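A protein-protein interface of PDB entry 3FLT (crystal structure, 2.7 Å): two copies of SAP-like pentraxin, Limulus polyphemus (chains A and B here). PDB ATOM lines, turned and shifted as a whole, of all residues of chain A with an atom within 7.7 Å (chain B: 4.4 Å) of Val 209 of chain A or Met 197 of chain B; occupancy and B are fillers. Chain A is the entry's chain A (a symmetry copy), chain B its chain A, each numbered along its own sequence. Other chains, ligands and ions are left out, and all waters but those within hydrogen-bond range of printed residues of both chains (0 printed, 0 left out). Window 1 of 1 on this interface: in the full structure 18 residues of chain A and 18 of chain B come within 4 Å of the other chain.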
ATOM      1  N   VAL A   2      16.964  -6.502   1.448  1.00  0.00           N
ATOM      2  CA  VAL A   2      18.267  -5.933   1.158  1.00  0.00           C
ATOM      3  C   VAL A   2      18.171  -5.372  -0.251  1.00  0.00           C
ATOM      4  O   VAL A   2      17.484  -5.942  -1.110  1.00  0.00           O
ATOM      5  CB  VAL A   2      19.360  -7.011   1.185  1.00  0.00           C
ATOM      6  CG1 VAL A   2      20.728  -6.376   1.024  1.00  0.00           C
ATOM      7  CG2 VAL A   2      19.268  -7.789   2.472  1.00  0.00           C
ATOM      8  N   ILE A   4      19.289  -4.761  -3.915  1.00  0.00           N
ATOM      9  CA  ILE A   4      20.064  -5.513  -4.881  1.00  0.00           C
ATOM     10  C   ILE A   4      21.466  -4.908  -5.102  1.00  0.00           C
ATOM     11  O   ILE A   4      22.389  -5.599  -5.535  1.00  0.00           O
ATOM     12  CB  ILE A   4      19.282  -5.578  -6.220  1.00  0.00           C
ATOM     13  CG1 ILE A   4      19.794  -6.715  -7.090  1.00  0.00           C
ATOM     14  CG2 ILE A   4      19.408  -4.259  -6.966  1.00  0.00           C
ATOM     15  CD1 ILE A   4      18.889  -6.997  -8.254  1.00  0.00           C
ATOM     16  N   ASP A   6      23.445  -4.042  -2.873  1.00  0.00           N
ATOM     17  CA  ASP A   6      24.330  -4.464  -1.801  1.00  0.00           C
ATOM     18  C   ASP A   6      24.947  -5.833  -2.056  1.00  0.00           C
ATOM     19  O   ASP A   6      25.665  -6.368  -1.211  1.00  0.00           O
ATOM     20  CB  ASP A   6      23.585  -4.452  -0.461  1.00  0.00           C
ATOM     21  CG  ASP A   6      23.248  -3.039   0.013  1.00  0.00           C
ATOM     22  OD1 ASP A   6      23.962  -2.080  -0.375  1.00  0.00           O
ATOM     23  OD2 ASP A   6      22.274  -2.891   0.790  1.00  0.00           O
ATOM     24  N   VAL A   7      24.664  -6.405  -3.221  1.00  0.00           N
ATOM     25  CA  VAL A   7      25.233  -7.700  -3.574  1.00  0.00           C
ATOM     26  C   VAL A   7      26.719  -7.442  -3.791  1.00  0.00           C
ATOM     27  O   VAL A   7      27.101  -6.399  -4.322  1.00  0.00           O
ATOM     28  CB  VAL A   7      24.613  -8.267  -4.881  1.00  0.00           C
ATOM     29  CG1 VAL A   7      25.398  -9.460  -5.354  1.00  0.00           C
ATOM     30  CG2 VAL A   7      23.176  -8.673  -4.646  1.00  0.00           C
ATOM     31  N   LYS A   8      27.566  -8.368  -3.364  1.00  0.00           N
ATOM     32  CA  LYS A   8      28.994  -8.180  -3.554  1.00  0.00           C
ATOM     33  C   LYS A   8      29.623  -9.431  -4.150  1.00  0.00           C
ATOM     34  O   LYS A   8      29.059 -10.522  -4.076  1.00  0.00           O
ATOM     35  CB  LYS A   8      29.678  -7.858  -2.224  1.00  0.00           C
ATOM     36  CG  LYS A   8      29.885  -9.065  -1.347  1.00  0.00           C
ATOM     37  CD  LYS A   8      30.645  -8.729  -0.073  1.00  0.00           C
ATOM     38  CE  LYS A   8      30.864  -9.999   0.748  1.00  0.00           C
ATOM     39  NZ  LYS A   8      31.363  -9.755   2.116  1.00  0.00           N
ATOM     40  N   ILE A   9      30.791  -9.256  -4.754  1.00  0.00           N
ATOM     41  CA  ILE A   9      31.514 -10.370  -5.338  1.00  0.00           C
ATOM     42  C   ILE A   9      32.870 -10.449  -4.646  1.00  0.00           C
ATOM     43  O   ILE A   9      33.531  -9.433  -4.439  1.00  0.00           O
ATOM     44  CB  ILE A   9      31.734 -10.169  -6.858  1.00  0.00           C
ATOM     45  CG1 ILE A   9      30.390 -10.168  -7.582  1.00  0.00           C
ATOM     46  CG2 ILE A   9      32.641 -11.266  -7.412  1.00  0.00           C
ATOM     47  CD1 ILE A   9      29.657 -11.458  -7.447  1.00  0.00           C
ATOM     48  N   SER A  10      33.275 -11.649  -4.259  1.00  0.00           N
ATOM     49  CA  SER A  10      34.575 -11.806  -3.629  1.00  0.00           C
ATOM     50  C   SER A  10      35.542 -12.405  -4.647  1.00  0.00           C
ATOM     51  O   SER A  10      35.215 -13.364  -5.353  1.00  0.00           O
ATOM     52  CB  SER A  10      34.491 -12.715  -2.394  1.00  0.00           C
ATOM     53  OG  SER A  10      33.746 -12.114  -1.344  1.00  0.00           O
ATOM     54  N   LEU A  22      35.144 -11.311 -13.439  1.00  0.00           N
ATOM     55  CA  LEU A  22      33.799 -11.078 -13.968  1.00  0.00           C
ATOM     56  C   LEU A  22      33.978 -10.515 -15.376  1.00  0.00           C
ATOM     57  O   LEU A  22      34.891  -9.720 -15.625  1.00  0.00           O
ATOM     58  CB  LEU A  22      33.040 -10.039 -13.132  1.00  0.00           C
ATOM     59  CG  LEU A  22      32.747 -10.237 -11.639  1.00  0.00           C
ATOM     60  CD1 LEU A  22      31.762  -9.161 -11.201  1.00  0.00           C
ATOM     61  CD2 LEU A  22      32.166 -11.621 -11.368  1.00  0.00           C
ATOM     62  N   MET A 197      24.334  -5.024 -10.936  1.00  0.00           N
ATOM     63  CA  MET A 197      23.213  -5.951 -10.885  1.00  0.00           C
ATOM     64  C   MET A 197      22.093  -5.663 -11.895  1.00  0.00           C
ATOM     65  O   MET A 197      21.052  -6.330 -11.884  1.00  0.00           O
ATOM     66  CB  MET A 197      22.650  -6.012  -9.463  1.00  0.00           C
ATOM     67  CG  MET A 197      23.656  -6.494  -8.431  1.00  0.00           C
ATOM     68  SD  MET A 197      24.546  -8.010  -8.916  1.00  0.00           S
ATOM     69  CE  MET A 197      23.365  -9.266  -8.456  1.00  0.00           C
ATOM     70  N   PHE A 201      26.560 -10.108 -16.214  1.00  0.00           N
ATOM     71  CA  PHE A 201      27.980 -10.380 -16.352  1.00  0.00           C
ATOM     72  C   PHE A 201      28.275 -11.852 -16.085  1.00  0.00           C
ATOM     73  O   PHE A 201      27.523 -12.530 -15.380  1.00  0.00           O
ATOM     74  CB  PHE A 201      28.778  -9.492 -15.389  1.00  0.00           C
ATOM     75  CG  PHE A 201      28.467  -9.721 -13.934  1.00  0.00           C
ATOM     76  CD1 PHE A 201      29.042 -10.781 -13.238  1.00  0.00           C
ATOM     77  CD2 PHE A 201      27.619  -8.855 -13.242  1.00  0.00           C
ATOM     78  CE1 PHE A 201      28.777 -10.971 -11.871  1.00  0.00           C
ATOM     79  CE2 PHE A 201      27.347  -9.032 -11.880  1.00  0.00           C
ATOM     80  CZ  PHE A 201      27.929 -10.090 -11.194  1.00  0.00           C
ATOM     81  N   ALA A 203      30.437 -14.895 -14.473  1.00  0.00           N
ATOM     82  CA  ALA A 203      31.240 -15.151 -13.282  1.00  0.00           C
ATOM     83  C   ALA A 203      32.052 -16.418 -13.517  1.00  0.00           C
ATOM     84  O   ALA A 203      31.512 -17.438 -13.946  1.00  0.00           O
ATOM     85  CB  ALA A 203      30.331 -15.319 -12.064  1.00  0.00           C
ATOM     86  N   GLY A 206      35.646 -19.371  -9.443  1.00  0.00           N
ATOM     87  CA  GLY A 206      35.398 -19.273  -8.021  1.00  0.00           C
ATOM     88  C   GLY A 206      35.100 -17.965  -7.325  1.00  0.00           C
ATOM     89  O   GLY A 206      35.323 -17.875  -6.117  1.00  0.00           O
ATOM     90  N   VAL A 207      34.617 -16.957  -8.041  1.00  0.00           N
ATOM     91  CA  VAL A 207      34.271 -15.704  -7.379  1.00  0.00           C
ATOM     92  C   VAL A 207      33.124 -16.063  -6.439  1.00  0.00           C
ATOM     93  O   VAL A 207      32.348 -16.972  -6.726  1.00  0.00           O
ATOM     94  CB  VAL A 207      33.783 -14.629  -8.384  1.00  0.00           C
ATOM     95  CG1 VAL A 207      34.912 -14.220  -9.305  1.00  0.00           C
ATOM     96  CG2 VAL A 207      32.614 -15.163  -9.184  1.00  0.00           C
ATOM     97  N   ILE A 208      33.009 -15.368  -5.318  1.00  0.00           N
ATOM     98  CA  ILE A 208      31.933 -15.664  -4.378  1.00  0.00           C
ATOM     99  C   ILE A 208      30.864 -14.579  -4.351  1.00  0.00           C
ATOM    100  O   ILE A 208      31.172 -13.397  -4.168  1.00  0.00           O
ATOM    101  CB  ILE A 208      32.468 -15.810  -2.956  1.00  0.00           C
ATOM    102  CG1 ILE A 208      33.676 -16.749  -2.948  1.00  0.00           C
ATOM    103  CG2 ILE A 208      31.357 -16.331  -2.046  1.00  0.00           C
ATOM    104  CD1 ILE A 208      34.312 -16.900  -1.596  1.00  0.00           C
ATOM    105  N   VAL A 209      29.611 -14.984  -4.528  1.00  0.00           N
ATOM    106  CA  VAL A 209      28.490 -14.048  -4.504  1.00  0.00           C
ATOM    107  C   VAL A 209      27.963 -13.937  -3.075  1.00  0.00           C
ATOM    108  O   VAL A 209      27.522 -14.925  -2.493  1.00  0.00           O
ATOM    109  CB  VAL A 209      27.342 -14.519  -5.413  1.00  0.00           C
ATOM    110  CG1 VAL A 209      26.196 -13.532  -5.349  1.00  0.00           C
ATOM    111  CG2 VAL A 209      27.835 -14.668  -6.823  1.00  0.00           C
ATOM    112  N   GLY A 210      28.016 -12.731  -2.518  1.00  0.00           N
ATOM    113  CA  GLY A 210      27.556 -12.512  -1.160  1.00  0.00           C
ATOM    114  C   GLY A 210      26.863 -11.174  -0.982  1.00  0.00           C
ATOM    115  O   GLY A 210      26.311 -10.616  -1.930  1.00  0.00           O
ATOM    116  N   ILE A 211      26.905 -10.645   0.236  1.00  0.00           N
ATOM    117  CA  ILE A 211      26.250  -9.378   0.550  1.00  0.00           C
ATOM    118  C   ILE A 211      27.173  -8.380   1.259  1.00  0.00           C
ATOM    119  O   ILE A 211      27.750  -8.697   2.289  1.00  0.00           O
ATOM    120  CB  ILE A 211      25.007  -9.629   1.458  1.00  0.00           C
ATOM    121  CG1 ILE A 211      23.957 -10.444   0.699  1.00  0.00           C
ATOM    122  CG2 ILE A 211      24.409  -8.304   1.919  1.00  0.00           C
ATOM    123  CD1 ILE A 211      23.362  -9.741  -0.514  1.00  0.00           C
ATOM    124  N   ILE B   4      16.201  -8.048  -4.574  1.00  0.00           N
ATOM    125  CA  ILE B   4      17.364  -8.910  -4.642  1.00  0.00           C
ATOM    126  C   ILE B   4      16.990 -10.370  -4.969  1.00  0.00           C
ATOM    127  O   ILE B   4      17.817 -11.135  -5.470  1.00  0.00           O
ATOM    128  CB  ILE B   4      18.133  -8.833  -3.296  1.00  0.00           C
ATOM    129  CG1 ILE B   4      19.565  -9.314  -3.463  1.00  0.00           C
ATOM    130  CG2 ILE B   4      17.426  -9.668  -2.240  1.00  0.00           C
ATOM    131  CD1 ILE B   4      20.421  -8.991  -2.273  1.00  0.00           C
ATOM    132  N   VAL B   7      17.272 -11.769  -8.707  1.00  0.00           N
ATOM    133  CA  VAL B   7      18.559 -12.019  -9.345  1.00  0.00           C
ATOM    134  C   VAL B   7      18.476 -13.444  -9.876  1.00  0.00           C
ATOM    135  O   VAL B   7      17.889 -14.317  -9.235  1.00  0.00           O
ATOM    136  CB  VAL B   7      19.735 -11.915  -8.334  1.00  0.00           C
ATOM    137  CG1 VAL B   7      21.004 -12.431  -8.957  1.00  0.00           C
ATOM    138  CG2 VAL B   7      19.934 -10.478  -7.908  1.00  0.00           C
ATOM    139  N   SER B 195      18.417 -19.126   1.716  1.00  0.00           N
ATOM    140  CA  SER B 195      17.556 -18.074   1.200  1.00  0.00           C
ATOM    141  C   SER B 195      18.321 -17.399   0.077  1.00  0.00           C
ATOM    142  O   SER B 195      19.398 -16.840   0.297  1.00  0.00           O
ATOM    143  CB  SER B 195      17.210 -17.057   2.291  1.00  0.00           C
ATOM    144  OG  SER B 195      16.361 -16.040   1.770  1.00  0.00           O
ATOM    145  N   TRP B 196      17.762 -17.469  -1.130  1.00  0.00           N
ATOM    146  CA  TRP B 196      18.376 -16.882  -2.319  1.00  0.00           C
ATOM    147  C   TRP B 196      18.992 -15.505  -2.067  1.00  0.00           C
ATOM    148  O   TRP B 196      18.330 -14.597  -1.573  1.00  0.00           O
ATOM    149  CB  TRP B 196      17.336 -16.771  -3.429  1.00  0.00           C
ATOM    150  CG  TRP B 196      17.908 -16.515  -4.775  1.00  0.00           C
ATOM    151  CD1 TRP B 196      17.546 -15.537  -5.646  1.00  0.00           C
ATOM    152  CD2 TRP B 196      18.923 -17.280  -5.428  1.00  0.00           C
ATOM    153  NE1 TRP B 196      18.273 -15.640  -6.811  1.00  0.00           N
ATOM    154  CE2 TRP B 196      19.125 -16.704  -6.703  1.00  0.00           C
ATOM    155  CE3 TRP B 196      19.683 -18.401  -5.063  1.00  0.00           C
ATOM    156  CZ2 TRP B 196      20.055 -17.211  -7.615  1.00  0.00           C
ATOM    157  CZ3 TRP B 196      20.608 -18.907  -5.969  1.00  0.00           C
ATOM    158  CH2 TRP B 196      20.786 -18.313  -7.231  1.00  0.00           C
ATOM    159  N   MET B 197      20.269 -15.369  -2.415  1.00  0.00           N
ATOM    160  CA  MET B 197      21.009 -14.126  -2.262  1.00  0.00           C
ATOM    161  C   MET B 197      21.299 -13.722  -0.810  1.00  0.00           C
ATOM    162  O   MET B 197      21.843 -12.642  -0.556  1.00  0.00           O
ATOM    163  CB  MET B 197      20.286 -12.995  -2.998  1.00  0.00           C
ATOM    164  CG  MET B 197      20.147 -13.234  -4.493  1.00  0.00           C
ATOM    165  SD  MET B 197      21.695 -13.747  -5.309  1.00  0.00           S
ATOM    166  CE  MET B 197      22.491 -12.170  -5.563  1.00  0.00           C
ATOM    167  N   GLU B 198      20.936 -14.576   0.145  1.00  0.00           N
ATOM    168  CA  GLU B 198      21.226 -14.282   1.546  1.00  0.00           C
ATOM    169  C   GLU B 198      22.231 -15.285   2.108  1.00  0.00           C
ATOM    170  O   GLU B 198      22.683 -15.157   3.245  1.00  0.00           O
ATOM    171  CB  GLU B 198      19.953 -14.278   2.395  1.00  0.00           C
ATOM    172  CG  GLU B 198      19.021 -13.121   2.081  1.00  0.00           C
ATOM    173  CD  GLU B 198      17.866 -13.009   3.062  1.00  0.00           C
ATOM    174  OE1 GLU B 198      17.266 -14.054   3.400  1.00  0.00           O
ATOM    175  OE2 GLU B 198      17.551 -11.873   3.487  1.00  0.00           O
ATOM    176  N   ASP B 199      22.576 -16.286   1.306  1.00  0.00           N
ATOM    177  CA  ASP B 199      23.548 -17.300   1.698  1.00  0.00           C
ATOM    178  C   ASP B 199      24.551 -17.362   0.571  1.00  0.00           C
ATOM    179  O   ASP B 199      24.230 -17.819  -0.526  1.00  0.00           O
ATOM    180  CB  ASP B 199      22.859 -18.646   1.881  1.00  0.00           C
ATOM    181  CG  ASP B 199      22.137 -18.744   3.204  1.00  0.00           C
ATOM    182  OD1 ASP B 199      22.828 -18.785   4.253  1.00  0.00           O
ATOM    183  OD2 ASP B 199      20.884 -18.769   3.198  1.00  0.00           O
ATOM    184  N   SER B 200      25.765 -16.894   0.842  1.00  0.00           N
ATOM    185  CA  SER B 200      26.795 -16.834  -0.183  1.00  0.00           C
ATOM    186  C   SER B 200      27.106 -18.166  -0.848  1.00  0.00           C
ATOM    187  O   SER B 200      27.033 -19.230  -0.223  1.00  0.00           O
ATOM    188  CB  SER B 200      28.062 -16.199   0.385  1.00  0.00           C
ATOM    189  OG  SER B 200      28.502 -16.895   1.527  1.00  0.00           O
ATOM    190  N   PHE B 201      27.423 -18.092  -2.140  1.00  0.00           N
ATOM    191  CA  PHE B 201      27.743 -19.269  -2.931  1.00  0.00           C
ATOM    192  C   PHE B 201      28.841 -18.956  -3.941  1.00  0.00           C
ATOM    193  O   PHE B 201      29.023 -17.804  -4.341  1.00  0.00           O
ATOM    194  CB  PHE B 201      26.484 -19.774  -3.648  1.00  0.00           C
ATOM    195  CG  PHE B 201      25.888 -18.789  -4.620  1.00  0.00           C
ATOM    196  CD1 PHE B 201      26.412 -18.644  -5.901  1.00  0.00           C
ATOM    197  CD2 PHE B 201      24.777 -18.024  -4.266  1.00  0.00           C
ATOM    198  CE1 PHE B 201      25.831 -17.750  -6.817  1.00  0.00           C
ATOM    199  CE2 PHE B 201      24.187 -17.130  -5.169  1.00  0.00           C
ATOM    200  CZ  PHE B 201      24.715 -16.996  -6.446  1.00  0.00           C
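The backbone carbonyl oxygen (O) of Phe 201 of chain B sits at hydrogen-bond distance from the backbone NH (N) of Val 209 of chain A.
O of Val 7 of chain B sits at hydrogen-bond distance from NE1 of Trp 196 of chain B (2.8 Å).
The backbone NH (N) of Ser 10 of chain A lies within hydrogen-bond range of the backbone carbonyl oxygen (O) of Ile 208 of chain A.
O of Val 2 of chain A touches CB of Ile 4 of chain B (3.7 Å).
Ile 4 of chain A touches Val 7 of chain B.
Val 7 of chain A touches Ile 4 of chain B.
CG2 of Val 7 of chain A touches CE of Met 197 of chain B, at 3.7 Å.
CE of Met 197 of chain A touches CG2 of Val 7 of chain B, 3.7 Å away.
Phe 201 of chain B touches Ile 208 of chain A.
CE of Met 197 of chain B touches CG1 of Val 209 of chain A, 3.95 Å away.
Val 209 of chain A touches Ser 200 of chain B.
Ile 211 of chain A touches Ile 4 of chain B.
Met 197 of chain B touches Ile 211 of chain A.
Val 209 of chain A touches just these residues of chain B: Met 197, Ser 200 and Phe 201.
Of chain A, only Val 7 (3.7 Å), Val 209 (3.95 Å) and Ile 211 (3.3 Å) come within 4 Å of Met 197 of chain B.
Printed residues of chain B within 4 Å of Ile 208 of chain A: Phe 201.
Printed residues of chain A within 4 Å of Val 7 of chain B: Ile 4 and Met 197.
Of the printed residues of chain B, Met 197 of chain A touches Val 7.
Ser 10 of chain A touches none of the printed residues of chain B.
The nearest printed residue of chain A that does not touch Ser 200 of chain B is Gly 210 of chain A (4.03 Å).
Of the 17 printed residues of chain A, 7 touch a printed residue of chain B.
Printed residues of chain A that touch a printed residue of chain B: Val 2, Ile 4, Val 7, Met 197, Ile 208, Val 209 and Ile 211.
Hydrophobic or aromatic side chains of chain A that line the printed part of chain B: Ile 4, Val 7, Met 197, Ile 208, Val 209 and Ile 211.
Among the printed residues, 11 pairs touch across the chains.
Ile 4 of chain A touches Val 7 of chain B, and with the chains exchanged Val 7 of chain A touches Ile 4 of chain B.
Val 7 of chain A touches Met 197 of chain B, and with the chains exchanged Met 197 of chain A touches Val 7 of chain B.
Positions printed for both chains: 4, 7, 197 and 201.
Of the 11 pairs that touch across the chains among the printed residues, 4 have their exchanged pair printed and touching as well.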
